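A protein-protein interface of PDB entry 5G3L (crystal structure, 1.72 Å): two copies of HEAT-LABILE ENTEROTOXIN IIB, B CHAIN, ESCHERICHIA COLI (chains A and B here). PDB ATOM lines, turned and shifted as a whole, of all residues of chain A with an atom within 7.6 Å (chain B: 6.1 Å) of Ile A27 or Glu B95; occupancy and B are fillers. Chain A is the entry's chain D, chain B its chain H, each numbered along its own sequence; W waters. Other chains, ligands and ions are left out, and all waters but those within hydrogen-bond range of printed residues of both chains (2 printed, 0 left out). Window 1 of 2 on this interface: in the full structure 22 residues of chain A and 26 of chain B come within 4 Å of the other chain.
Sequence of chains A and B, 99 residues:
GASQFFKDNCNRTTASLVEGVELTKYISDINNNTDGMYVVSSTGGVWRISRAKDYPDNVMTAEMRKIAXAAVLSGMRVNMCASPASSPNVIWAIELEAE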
ATOM      1  N   THR A  24       2.616  -9.586  15.155  1.00  0.00           N
ATOM      2  CA  THR A  24       1.377  -8.831  15.176  1.00  0.00           C
ATOM      3  C   THR A  24       0.671  -8.791  16.548  1.00  0.00           C
ATOM      4  O   THR A  24      -0.173  -7.929  16.742  1.00  0.00           O
ATOM      5  CB  THR A  24       0.365  -9.337  14.128  1.00  0.00           C
ATOM      6  OG1 THR A  24       0.064 -10.668  14.401  1.00  0.00           O
ATOM      7  CG2 THR A  24       0.981  -9.180  12.715  1.00  0.00           C
ATOM      8  N   LYS A  25       1.124  -9.605  17.498  1.00  0.00           N
ATOM      9  CA  LYS A  25       0.638  -9.554  18.877  1.00  0.00           C
ATOM     10  C   LYS A  25       1.747  -9.735  19.913  1.00  0.00           C
ATOM     11  O   LYS A  25       2.724 -10.462  19.689  1.00  0.00           O
ATOM     12  CB  LYS A  25      -0.432 -10.612  19.103  1.00  0.00           C
ATOM     13  CG  LYS A  25      -1.548 -10.580  18.010  1.00  0.00           C
ATOM     14  CD  LYS A  25      -2.786 -11.278  18.376  1.00  0.00           C
ATOM     15  CE  LYS A  25      -3.696 -11.595  17.193  1.00  0.00           C
ATOM     16  NZ  LYS A  25      -4.454 -10.418  16.718  1.00  0.00           N
ATOM     17  N   TYR A  26       1.591  -9.063  21.044  1.00  0.00           N
ATOM     18  CA  TYR A  26       2.518  -9.144  22.172  1.00  0.00           C
ATOM     19  C   TYR A  26       1.708  -9.373  23.437  1.00  0.00           C
ATOM     20  O   TYR A  26       0.749  -8.618  23.698  1.00  0.00           O
ATOM     21  CB  TYR A  26       3.250  -7.834  22.289  1.00  0.00           C
ATOM     22  CG  TYR A  26       4.304  -7.723  23.358  1.00  0.00           C
ATOM     23  CD1 TYR A  26       5.315  -8.680  23.499  1.00  0.00           C
ATOM     24  CD2 TYR A  26       4.355  -6.639  24.197  1.00  0.00           C
ATOM     25  CE1 TYR A  26       6.346  -8.523  24.434  1.00  0.00           C
ATOM     26  CE2 TYR A  26       5.365  -6.487  25.136  1.00  0.00           C
ATOM     27  CZ  TYR A  26       6.348  -7.435  25.273  1.00  0.00           C
ATOM     28  OH  TYR A  26       7.375  -7.337  26.216  1.00  0.00           O
ATOM     29  N   ILE A  27       2.050 -10.425  24.154  1.00  0.00           N
ATOM     30  CA  ILE A  27       1.273 -10.930  25.329  1.00  0.00           C
ATOM     31  C   ILE A  27       2.064 -10.879  26.613  1.00  0.00           C
ATOM     32  O   ILE A  27       3.202 -11.421  26.679  1.00  0.00           O
ATOM     33  CB  ILE A  27       0.808 -12.390  25.121  1.00  0.00           C
ATOM     34  CG1 ILE A  27      -0.091 -12.520  23.891  1.00  0.00           C
ATOM     35  CG2 ILE A  27       0.052 -12.847  26.367  1.00  0.00           C
ATOM     36  CD1 ILE A  27      -0.347 -13.982  23.447  1.00  0.00           C
ATOM     37  N   SER A  28       1.446 -10.322  27.686  1.00  0.00           N
ATOM     38  CA  SER A  28       1.921 -10.469  29.051  1.00  0.00           C
ATOM     39  C   SER A  28       0.878 -11.207  29.880  1.00  0.00           C
ATOM     40  O   SER A  28      -0.273 -10.818  29.858  1.00  0.00           O
ATOM     41  CB  SER A  28       2.221  -9.107  29.687  1.00  0.00           C
ATOM     42  OG  SER A  28       2.569  -9.297  31.031  1.00  0.00           O
ATOM     43  N   ASP A  29       1.302 -12.286  30.514  1.00  0.00           N
ATOM     44  CA  ASP A  29       0.377 -13.182  31.245  1.00  0.00           C
ATOM     45  C   ASP A  29       0.922 -13.512  32.617  1.00  0.00           C
ATOM     46  O   ASP A  29       2.081 -13.934  32.747  1.00  0.00           O
ATOM     47  CB  ASP A  29       0.172 -14.419  30.364  1.00  0.00           C
ATOM     48  CG  ASP A  29      -0.838 -15.417  30.887  1.00  0.00           C
ATOM     49  OD1 ASP A  29      -1.039 -15.546  32.110  1.00  0.00           O
ATOM     50  OD2 ASP A  29      -1.458 -16.132  30.034  1.00  0.00           O
ATOM     51  N   ILE A  30       0.103 -13.302  33.674  1.00  0.00           N
ATOM     52  CA  ILE A  30       0.518 -13.691  35.037  1.00  0.00           C
ATOM     53  C   ILE A  30      -0.324 -14.837  35.634  1.00  0.00           C
ATOM     54  O   ILE A  30      -0.202 -15.139  36.810  1.00  0.00           O
ATOM     55  CB  ILE A  30       0.587 -12.550  36.034  1.00  0.00           C
ATOM     56  CG1 ILE A  30      -0.780 -11.851  36.193  1.00  0.00           C
ATOM     57  CG2 ILE A  30       1.671 -11.573  35.617  1.00  0.00           C
ATOM     58  CD1 ILE A  30      -0.782 -11.012  37.483  1.00  0.00           C
ATOM     59  N   THR A  34       0.354 -20.469  32.823  1.00  0.00           N
ATOM     60  CA  THR A  34       0.554 -19.839  31.541  1.00  0.00           C
ATOM     61  C   THR A  34       1.383 -18.562  31.615  1.00  0.00           C
ATOM     62  O   THR A  34       1.576 -17.872  30.612  1.00  0.00           O
ATOM     63  CB  THR A  34      -0.752 -19.546  30.816  1.00  0.00           C
ATOM     64  OG1 THR A  34      -1.551 -18.665  31.609  1.00  0.00           O
ATOM     65  CG2 THR A  34      -1.499 -20.831  30.554  1.00  0.00           C
ATOM     66  N   GLY A  36       4.024 -15.722  31.593  1.00  0.00           N
ATOM     67  CA  GLY A  36       5.156 -15.437  30.734  1.00  0.00           C
ATOM     68  C   GLY A  36       4.914 -14.322  29.779  1.00  0.00           C
ATOM     69  O   GLY A  36       3.834 -13.674  29.784  1.00  0.00           O
ATOM     70  N   MET A  37       5.916 -14.104  28.925  1.00  0.00           N
ATOM     71  CA  MET A  37       5.857 -13.142  27.861  1.00  0.00           C
ATOM     72  C   MET A  37       5.947 -13.855  26.504  1.00  0.00           C
ATOM     73  O   MET A  37       6.793 -14.724  26.351  1.00  0.00           O
ATOM     74  CB  MET A  37       7.001 -12.124  27.914  1.00  0.00           C
ATOM     75  CG  MET A  37       7.046 -11.301  29.215  1.00  0.00           C
ATOM     76  SD  MET A  37       5.609 -10.240  29.406  1.00  0.00           S
ATOM     77  CE  MET A  37       5.513  -9.392  27.847  1.00  0.00           C
ATOM     78  N   TYR A  38       5.044 -13.528  25.586  1.00  0.00           N
ATOM     79  CA  TYR A  38       4.923 -14.201  24.294  1.00  0.00           C
ATOM     80  C   TYR A  38       4.758 -13.240  23.159  1.00  0.00           C
ATOM     81  O   TYR A  38       4.204 -12.121  23.301  1.00  0.00           O
ATOM     82  CB  TYR A  38       3.759 -15.222  24.315  1.00  0.00           C
ATOM     83  CG  TYR A  38       3.683 -16.137  25.500  1.00  0.00           C
ATOM     84  CD1 TYR A  38       2.994 -15.771  26.657  1.00  0.00           C
ATOM     85  CD2 TYR A  38       4.293 -17.420  25.505  1.00  0.00           C
ATOM     86  CE1 TYR A  38       2.892 -16.622  27.733  1.00  0.00           C
ATOM     87  CE2 TYR A  38       4.221 -18.247  26.587  1.00  0.00           C
ATOM     88  CZ  TYR A  38       3.469 -17.908  27.690  1.00  0.00           C
ATOM     89  OH  TYR A  38       3.327 -18.815  28.746  1.00  0.00           O
ATOM     90  N   VAL A  39       5.121 -13.712  21.973  1.00  0.00           N
ATOM     91  CA  VAL A  39       4.796 -13.052  20.761  1.00  0.00           C
ATOM     92  C   VAL A  39       4.046 -13.983  19.786  1.00  0.00           C
ATOM     93  O   VAL A  39       4.229 -15.197  19.827  1.00  0.00           O
ATOM     94  CB  VAL A  39       6.028 -12.469  20.020  1.00  0.00           C
ATOM     95  CG1 VAL A  39       6.689 -11.383  20.884  1.00  0.00           C
ATOM     96  CG2 VAL A  39       7.031 -13.551  19.653  1.00  0.00           C
ATOM     97  N   VAL A  40       3.209 -13.378  18.981  1.00  0.00           N
ATOM     98  CA  VAL A  40       2.402 -14.084  17.951  1.00  0.00           C
ATOM     99  C   VAL A  40       2.693 -13.456  16.587  1.00  0.00           C
ATOM    100  O   VAL A  40       2.646 -12.234  16.405  1.00  0.00           O
ATOM    101  CB  VAL A  40       0.886 -14.022  18.229  1.00  0.00           C
ATOM    102  CG1 VAL A  40       0.147 -14.990  17.294  1.00  0.00           C
ATOM    103  CG2 VAL A  40       0.560 -14.395  19.695  1.00  0.00           C
ATOM    104  N   VAL A  46       3.362 -18.940  17.647  1.00  0.00           N
ATOM    105  CA  VAL A  46       3.584 -18.416  19.025  1.00  0.00           C
ATOM    106  C   VAL A  46       4.968 -18.808  19.553  1.00  0.00           C
ATOM    107  O   VAL A  46       5.381 -19.942  19.444  1.00  0.00           O
ATOM    108  CB  VAL A  46       2.543 -18.985  19.980  1.00  0.00           C
ATOM    109  CG1 VAL A  46       2.666 -18.343  21.380  1.00  0.00           C
ATOM    110  CG2 VAL A  46       1.170 -18.772  19.419  1.00  0.00           C
ATOM    111  N   TRP A  47       5.669 -17.852  20.168  1.00  0.00           N
ATOM    112  CA  TRP A  47       6.957 -18.056  20.788  1.00  0.00           C
ATOM    113  C   TRP A  47       6.996 -17.404  22.191  1.00  0.00           C
ATOM    114  O   TRP A  47       6.329 -16.395  22.395  1.00  0.00           O
ATOM    115  CB  TRP A  47       8.108 -17.436  19.965  1.00  0.00           C
ATOM    116  CG  TRP A  47       8.366 -18.072  18.682  1.00  0.00           C
ATOM    117  CD1 TRP A  47       9.332 -19.039  18.414  1.00  0.00           C
ATOM    118  CD2 TRP A  47       7.719 -17.821  17.440  1.00  0.00           C
ATOM    119  NE1 TRP A  47       9.289 -19.396  17.102  1.00  0.00           N
ATOM    120  CE2 TRP A  47       8.347 -18.641  16.468  1.00  0.00           C
ATOM    121  CE3 TRP A  47       6.734 -16.948  17.017  1.00  0.00           C
ATOM    122  CZ2 TRP A  47       7.917 -18.673  15.153  1.00  0.00           C
ATOM    123  CZ3 TRP A  47       6.312 -16.980  15.712  1.00  0.00           C
ATOM    124  CH2 TRP A  47       6.905 -17.825  14.794  1.00  0.00           C
ATOM    125  N   ILE A  49       9.227 -15.631  25.027  1.00  0.00           N
ATOM    126  CA  ILE A  49      10.432 -14.868  25.281  1.00  0.00           C
ATOM    127  C   ILE A  49      11.114 -15.440  26.530  1.00  0.00           C
ATOM    128  O   ILE A  49      10.522 -15.595  27.554  1.00  0.00           O
ATOM    129  CB  ILE A  49      10.168 -13.353  25.401  1.00  0.00           C
ATOM    130  CG1 ILE A  49       9.447 -12.840  24.161  1.00  0.00           C
ATOM    131  CG2 ILE A  49      11.448 -12.603  25.654  1.00  0.00           C
ATOM    132  CD1 ILE A  49       8.986 -11.404  24.256  1.00  0.00           C
ATOM    133  N   ALA A  68      10.575  -7.033  20.788  1.00  0.00           N
ATOM    134  CA  ALA A  68       9.216  -7.541  20.488  1.00  0.00           C
ATOM    135  C   ALA A  68       8.218  -6.421  20.403  1.00  0.00           C
ATOM    136  O   ALA A  68       7.422  -6.350  19.463  1.00  0.00           O
ATOM    137  CB  ALA A  68       8.811  -8.572  21.558  1.00  0.00           C
ATOM    138  N   VAL A  72       6.141  -5.069  17.027  1.00  0.00           N
ATOM    139  CA  VAL A  72       4.658  -5.042  16.977  1.00  0.00           C
ATOM    140  C   VAL A  72       4.183  -3.634  16.614  1.00  0.00           C
ATOM    141  O   VAL A  72       3.318  -3.443  15.730  1.00  0.00           O
ATOM    142  CB  VAL A  72       4.032  -5.599  18.270  1.00  0.00           C
ATOM    143  CG1 VAL A  72       2.519  -5.275  18.326  1.00  0.00           C
ATOM    144  CG2 VAL A  72       4.269  -7.112  18.357  1.00  0.00           C
ATOM    145  N   GLY B   1      -8.844 -10.016  15.923  1.00  0.00           N
ATOM    146  CA  GLY B   1      -9.288 -10.724  17.169  1.00  0.00           C
ATOM    147  C   GLY B   1      -8.149 -11.334  17.980  1.00  0.00           C
ATOM    148  O   GLY B   1      -7.042 -11.521  17.476  1.00  0.00           O
ATOM    149  N   ALA B   2      -8.467 -11.737  19.192  1.00  0.00           N
ATOM    150  CA  ALA B   2      -7.501 -12.347  20.106  1.00  0.00           C
ATOM    151  C   ALA B   2      -6.966 -13.639  19.477  1.00  0.00           C
ATOM    152  O   ALA B   2      -7.668 -14.369  18.772  1.00  0.00           O
ATOM    153  CB  ALA B   2      -8.118 -12.667  21.455  1.00  0.00           C
ATOM    154  N   SER B   3      -5.689 -13.881  19.697  1.00  0.00           N
ATOM    155  CA  SER B   3      -5.085 -15.107  19.225  1.00  0.00           C
ATOM    156  C   SER B   3      -5.739 -16.336  19.892  1.00  0.00           C
ATOM    157  O   SER B   3      -6.213 -16.260  21.026  1.00  0.00           O
ATOM    158  CB  SER B   3      -3.569 -15.124  19.527  1.00  0.00           C
ATOM    159  OG  SER B   3      -3.267 -15.148  20.889  1.00  0.00           O
ATOM    160  N   PHE B   5      -4.228 -18.839  21.086  1.00  0.00           N
ATOM    161  CA  PHE B   5      -3.420 -19.049  22.272  1.00  0.00           C
ATOM    162  C   PHE B   5      -3.901 -18.220  23.495  1.00  0.00           C
ATOM    163  O   PHE B   5      -4.098 -18.757  24.582  1.00  0.00           O
ATOM    164  CB  PHE B   5      -1.956 -18.713  21.922  1.00  0.00           C
ATOM    165  CG  PHE B   5      -0.981 -18.847  23.049  1.00  0.00           C
ATOM    166  CD1 PHE B   5      -0.527 -20.085  23.474  1.00  0.00           C
ATOM    167  CD2 PHE B   5      -0.460 -17.683  23.691  1.00  0.00           C
ATOM    168  CE1 PHE B   5       0.367 -20.211  24.493  1.00  0.00           C
ATOM    169  CE2 PHE B   5       0.505 -17.827  24.651  1.00  0.00           C
ATOM    170  CZ  PHE B   5       0.935 -19.068  25.070  1.00  0.00           C
ATOM    171  N   PHE B   6      -4.086 -16.927  23.264  1.00  0.00           N
ATOM    172  CA  PHE B   6      -4.576 -16.028  24.315  1.00  0.00           C
ATOM    173  C   PHE B   6      -5.941 -16.448  24.852  1.00  0.00           C
ATOM    174  O   PHE B   6      -6.171 -16.520  26.044  1.00  0.00           O
ATOM    175  CB  PHE B   6      -4.566 -14.591  23.826  1.00  0.00           C
ATOM    176  CG  PHE B   6      -4.819 -13.591  24.909  1.00  0.00           C
ATOM    177  CD1 PHE B   6      -3.797 -13.112  25.675  1.00  0.00           C
ATOM    178  CD2 PHE B   6      -6.110 -13.131  25.151  1.00  0.00           C
ATOM    179  CE1 PHE B   6      -4.019 -12.152  26.662  1.00  0.00           C
ATOM    180  CE2 PHE B   6      -6.360 -12.188  26.140  1.00  0.00           C
ATOM    181  CZ  PHE B   6      -5.301 -11.722  26.936  1.00  0.00           C
ATOM    182  N   ASN B   9      -5.736 -19.819  26.912  1.00  0.00           N
ATOM    183  CA  ASN B   9      -5.165 -19.538  28.208  1.00  0.00           C
ATOM    184  C   ASN B   9      -6.191 -18.847  29.181  1.00  0.00           C
ATOM    185  O   ASN B   9      -6.319 -19.241  30.320  1.00  0.00           O
ATOM    186  CB  ASN B   9      -3.901 -18.695  28.105  1.00  0.00           C
ATOM    187  CG  ASN B   9      -2.777 -19.409  27.372  1.00  0.00           C
ATOM    188  OD1 ASN B   9      -2.758 -20.637  27.275  1.00  0.00           O
ATOM    189  ND2 ASN B   9      -1.818 -18.635  26.901  1.00  0.00           N
ATOM    190  N   ILE B  67       2.441  -1.999  27.628  1.00  0.00           N
ATOM    191  CA  ILE B  67       1.397  -2.280  26.651  1.00  0.00           C
ATOM    192  C   ILE B  67       0.259  -1.217  26.771  1.00  0.00           C
ATOM    193  O   ILE B  67      -0.232  -0.656  25.765  1.00  0.00           O
ATOM    194  CB  ILE B  67       0.863  -3.711  26.823  1.00  0.00           C
ATOM    195  CG1 ILE B  67       1.876  -4.724  26.255  1.00  0.00           C
ATOM    196  CG2 ILE B  67      -0.492  -3.887  26.163  1.00  0.00           C
ATOM    197  CD1 ILE B  67       1.632  -6.170  26.672  1.00  0.00           C
ATOM    198  N   ARG B  77      -5.487  -1.653  19.452  1.00  0.00           N
ATOM    199  CA  ARG B  77      -6.414  -2.381  20.321  1.00  0.00           C
ATOM    200  C   ARG B  77      -5.707  -3.391  21.181  1.00  0.00           C
ATOM    201  O   ARG B  77      -4.608  -3.827  20.889  1.00  0.00           O
ATOM    202  CB  ARG B  77      -7.500  -3.100  19.490  1.00  0.00           C
ATOM    203  CG  ARG B  77      -8.244  -2.228  18.525  1.00  0.00           C
ATOM    204  CD  ARG B  77      -9.073  -1.217  19.269  1.00  0.00           C
ATOM    205  NE  ARG B  77      -9.635  -0.137  18.474  1.00  0.00           N
ATOM    206  CZ  ARG B  77     -10.906  -0.017  18.076  1.00  0.00           C
ATOM    207  NH1 ARG B  77     -11.818  -0.959  18.324  1.00  0.00           N
ATOM    208  NH2 ARG B  77     -11.257   1.078  17.394  1.00  0.00           N
ATOM    209  N   VAL B  78      -6.365  -3.745  22.267  1.00  0.00           N
ATOM    210  CA  VAL B  78      -5.903  -4.811  23.174  1.00  0.00           C
ATOM    211  C   VAL B  78      -7.014  -5.840  23.403  1.00  0.00           C
ATOM    212  O   VAL B  78      -8.219  -5.554  23.338  1.00  0.00           O
ATOM    213  CB  VAL B  78      -5.419  -4.303  24.565  1.00  0.00           C
ATOM    214  CG1 VAL B  78      -4.288  -3.292  24.402  1.00  0.00           C
ATOM    215  CG2 VAL B  78      -6.547  -3.656  25.353  1.00  0.00           C
ATOM    216  N   ASN B  79      -6.582  -7.052  23.716  1.00  0.00           N
ATOM    217  CA  ASN B  79      -7.447  -8.091  24.292  1.00  0.00           C
ATOM    218  C   ASN B  79      -7.037  -8.341  25.729  1.00  0.00           C
ATOM    219  O   ASN B  79      -5.848  -8.386  26.030  1.00  0.00           O
ATOM    220  CB  ASN B  79      -7.342  -9.372  23.445  1.00  0.00           C
ATOM    221  CG  ASN B  79      -7.468  -9.063  21.965  1.00  0.00           C
ATOM    222  OD1 ASN B  79      -8.472  -8.518  21.524  1.00  0.00           O
ATOM    223  ND2 ASN B  79      -6.431  -9.410  21.179  1.00  0.00           N
ATOM    224  N   MET B  80      -8.010  -8.484  26.627  1.00  0.00           N
ATOM    225  CA  MET B  80      -7.728  -8.644  28.049  1.00  0.00           C
ATOM    226  C   MET B  80      -8.350  -9.946  28.588  1.00  0.00           C
ATOM    227  O   MET B  80      -9.404 -10.345  28.121  1.00  0.00           O
ATOM    228  CB  MET B  80      -8.205  -7.433  28.847  1.00  0.00           C
ATOM    229  CG  MET B  80      -7.331  -6.200  28.591  1.00  0.00           C
ATOM    230  SD  MET B  80      -7.819  -4.704  29.410  1.00  0.00           S
ATOM    231  CE  MET B  80      -9.384  -4.464  28.634  1.00  0.00           C
ATOM    232  N   ALA B  93      -4.026 -11.055  32.136  1.00  0.00           N
ATOM    233  CA  ALA B  93      -3.253 -11.158  30.884  1.00  0.00           C
ATOM    234  C   ALA B  93      -3.756 -10.112  29.934  1.00  0.00           C
ATOM    235  O   ALA B  93      -4.936  -9.728  29.929  1.00  0.00           O
ATOM    236  CB  ALA B  93      -3.383 -12.555  30.272  1.00  0.00           C
ATOM    237  N   ILE B  94      -2.851  -9.648  29.083  1.00  0.00           N
ATOM    238  CA  ILE B  94      -3.178  -8.666  28.086  1.00  0.00           C
ATOM    239  C   ILE B  94      -2.375  -8.916  26.806  1.00  0.00           C
ATOM    240  O   ILE B  94      -1.205  -9.346  26.860  1.00  0.00           O
ATOM    241  CB  ILE B  94      -2.984  -7.197  28.653  1.00  0.00           C
ATOM    242  CG1 ILE B  94      -3.489  -6.157  27.655  1.00  0.00           C
ATOM    243  CG2 ILE B  94      -1.529  -6.950  28.995  1.00  0.00           C
ATOM    244  CD1 ILE B  94      -3.714  -4.757  28.252  1.00  0.00           C
ATOM    245  N   GLU B  95      -3.026  -8.673  25.677  1.00  0.00           N
ATOM    246  CA  GLU B  95      -2.503  -8.864  24.317  1.00  0.00           C
ATOM    247  C   GLU B  95      -2.651  -7.574  23.512  1.00  0.00           C
ATOM    248  O   GLU B  95      -3.748  -7.121  23.255  1.00  0.00           O
ATOM    249  CB  GLU B  95      -3.223 -10.027  23.603  1.00  0.00           C
ATOM    250  CG  GLU B  95      -2.751 -10.331  22.194  1.00  0.00           C
ATOM    251  CD  GLU B  95      -3.384 -11.637  21.678  1.00  0.00           C
ATOM    252  OE1 GLU B  95      -4.599 -11.625  21.437  1.00  0.00           O
ATOM    253  OE2 GLU B  95      -2.635 -12.633  21.488  1.00  0.00           O
ATOM    254  N   LEU B  96      -1.513  -6.973  23.144  1.00  0.00           N
ATOM    255  CA  LEU B  96      -1.470  -5.799  22.266  1.00  0.00           C
ATOM    256  C   LEU B  96      -1.499  -6.266  20.816  1.00  0.00           C
ATOM    257  O   LEU B  96      -0.730  -7.154  20.463  1.00  0.00           O
ATOM    258  CB  LEU B  96      -0.172  -5.035  22.481  1.00  0.00           C
ATOM    259  CG  LEU B  96       0.042  -3.740  21.660  1.00  0.00           C
ATOM    260  CD1 LEU B  96      -0.973  -2.694  21.978  1.00  0.00           C
ATOM    261  CD2 LEU B  96       1.451  -3.218  21.940  1.00  0.00           C
ATOM    262  N   GLU B  97      -2.374  -5.692  20.009  1.00  0.00           N
ATOM    263  CA  GLU B  97      -2.443  -6.139  18.600  1.00  0.00           C
ATOM    264  C   GLU B  97      -2.255  -5.023  17.584  1.00  0.00           C
ATOM    265  O   GLU B  97      -2.769  -3.895  17.720  1.00  0.00           O
ATOM    266  CB  GLU B  97      -3.678  -7.010  18.323  1.00  0.00           C
ATOM    267  CG  GLU B  97      -4.979  -6.389  18.559  1.00  0.00           C
ATOM    268  CD  GLU B  97      -6.145  -7.268  18.096  1.00  0.00           C
ATOM    269  OE1 GLU B  97      -6.218  -8.497  18.321  1.00  0.00           O
ATOM    270  OE2 GLU B  97      -7.041  -6.681  17.531  1.00  0.00           O
HETATM  271  O   HOH W   1      -4.147 -19.461  32.260  1.00  0.00           O
HETATM  272  O   HOH W   2      -2.182 -15.764  27.348  1.00  0.00           O
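NZ of Lys A25 lies within hydrogen-bond range of O of Gly B1, 2.9 Å away.
NZ of Lys A25 lies within salt-bridge range of OE1 of Glu B97 (3.1 Å).
The backbone carbonyl oxygen of Tyr A26 is in hydrogen-bond range of the backbone NH of Leu B96, 2.9 Å away.
O of Ser A28 lies within hydrogen-bond range of N of Ile B94 (2.9 Å).
OG1 of Thr A34 sits at hydrogen-bond distance from OD2 of Asp A29 (3.0 Å).
The backbone NH (N) of Gly A36 sits at hydrogen-bond distance from the backbone carbonyl oxygen (O) of Asp A29, at 2.9 Å.
O of Thr A34 sits at hydrogen-bond distance from OH of Tyr A38 (2.7 Å).
The side-chain hydroxyl of Ser B3 lies within hydrogen-bond range of the side-chain carboxylate of Glu B95 (2.7 Å).
O of Phe B5 sits close to ND2 of Asn B9.
The backbone carbonyl oxygen of Arg B77 is in hydrogen-bond range of the backbone NH of Glu B97, 3.0 Å away.
Among the printed residues, merely in contact across the chains: Ser A28 with Ala B93 (3.2 Å), Lys A25 with Leu B96 (3.2 Å), Ile A27 with Glu B95 (3.3 Å), Ile A27 with Ile B94 (3.3 Å), Tyr A26 with Glu B95 (3.3 Å), Lys A25 with Glu B95 (3.4 Å), Thr A24 with Glu B97 (3.4 Å), Thr A34 with Asn B9 (3.5 Å), Tyr A38 with Phe B5 (3.7 Å), Tyr A26 with Ile B67 (3.7 Å), Ile A27 with Phe B5 (3.7 Å), Tyr A26 with Ile B94 (3.8 Å), Thr A24 with Leu B96 (3.8 Å), Asp A29 with Ala B93 (3.9 Å), Ile A27 with Phe B6 (3.9 Å), Lys A25 with Ser B3 (3.9 Å) and Val A46 with Phe B5 (3.9 Å).
Printed residues of chain B within 4 Å of Lys A25: Gly B1 (2.9 Å), Ser B3 (3.9 Å), Glu B95 (3.4 Å), Leu B96 (3.2 Å) and Glu B97 (3.1 Å).
Of chain B, only Phe B5, Phe B6, Ile B94 and Glu B95 come within 4 Å of Ile A27.
Of the printed residues of chain A, Gly B1 touches Lys A25.
Printed residues of chain A within 4 Å of Asn B9: Thr A34.
Glu B95 touches just these residues of chain A: Lys A25, Tyr A26 and Ile A27.
The nearest residue of chain A that does not touch Glu B95 is Val A40 (4.1 Å).
The nearest printed residue of chain A that does not touch Ser B3 is Ile A27 (4.1 Å).
Printed residues of chain B that touch a printed residue of chain A: Gly B1, Ser B3, Phe B5, Phe B6, Asn B9, Ile B67, Ala B93, Ile B94, Glu B95, Leu B96 and Glu B97.
Hydrophobic or aromatic side chains of chain B within 4 Å of the printed part of chain A: Phe B5, Phe B6, Ile B67, Ala B93 and Leu B96.
Of the 18 printed residues of chain A, 9 touch a printed residue of chain B.
Among the printed residues, 21 pairs touch across the chains.
Among the printed residues, Asp or Glu carboxylates within 4 Å of a Lys or Arg side-chain nitrogen of the other chain: Lys A25 with Glu B97.
No position is printed for both chains.
Of the 21 pairs that touch across the chains among the printed residues, none has its exchanged pair printed and touching as well.
Water W1 lies within hydrogen-bond range of the side-chain hydroxyl (OG1) of Thr A34 (2.8 Å) and the backbone carbonyl oxygen (O) of Asn B9 (2.9 Å).
Water W2 bridges OD2 of Asp A29 (2.8 Å) and ND2 of Asn B9 (2.9 Å).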
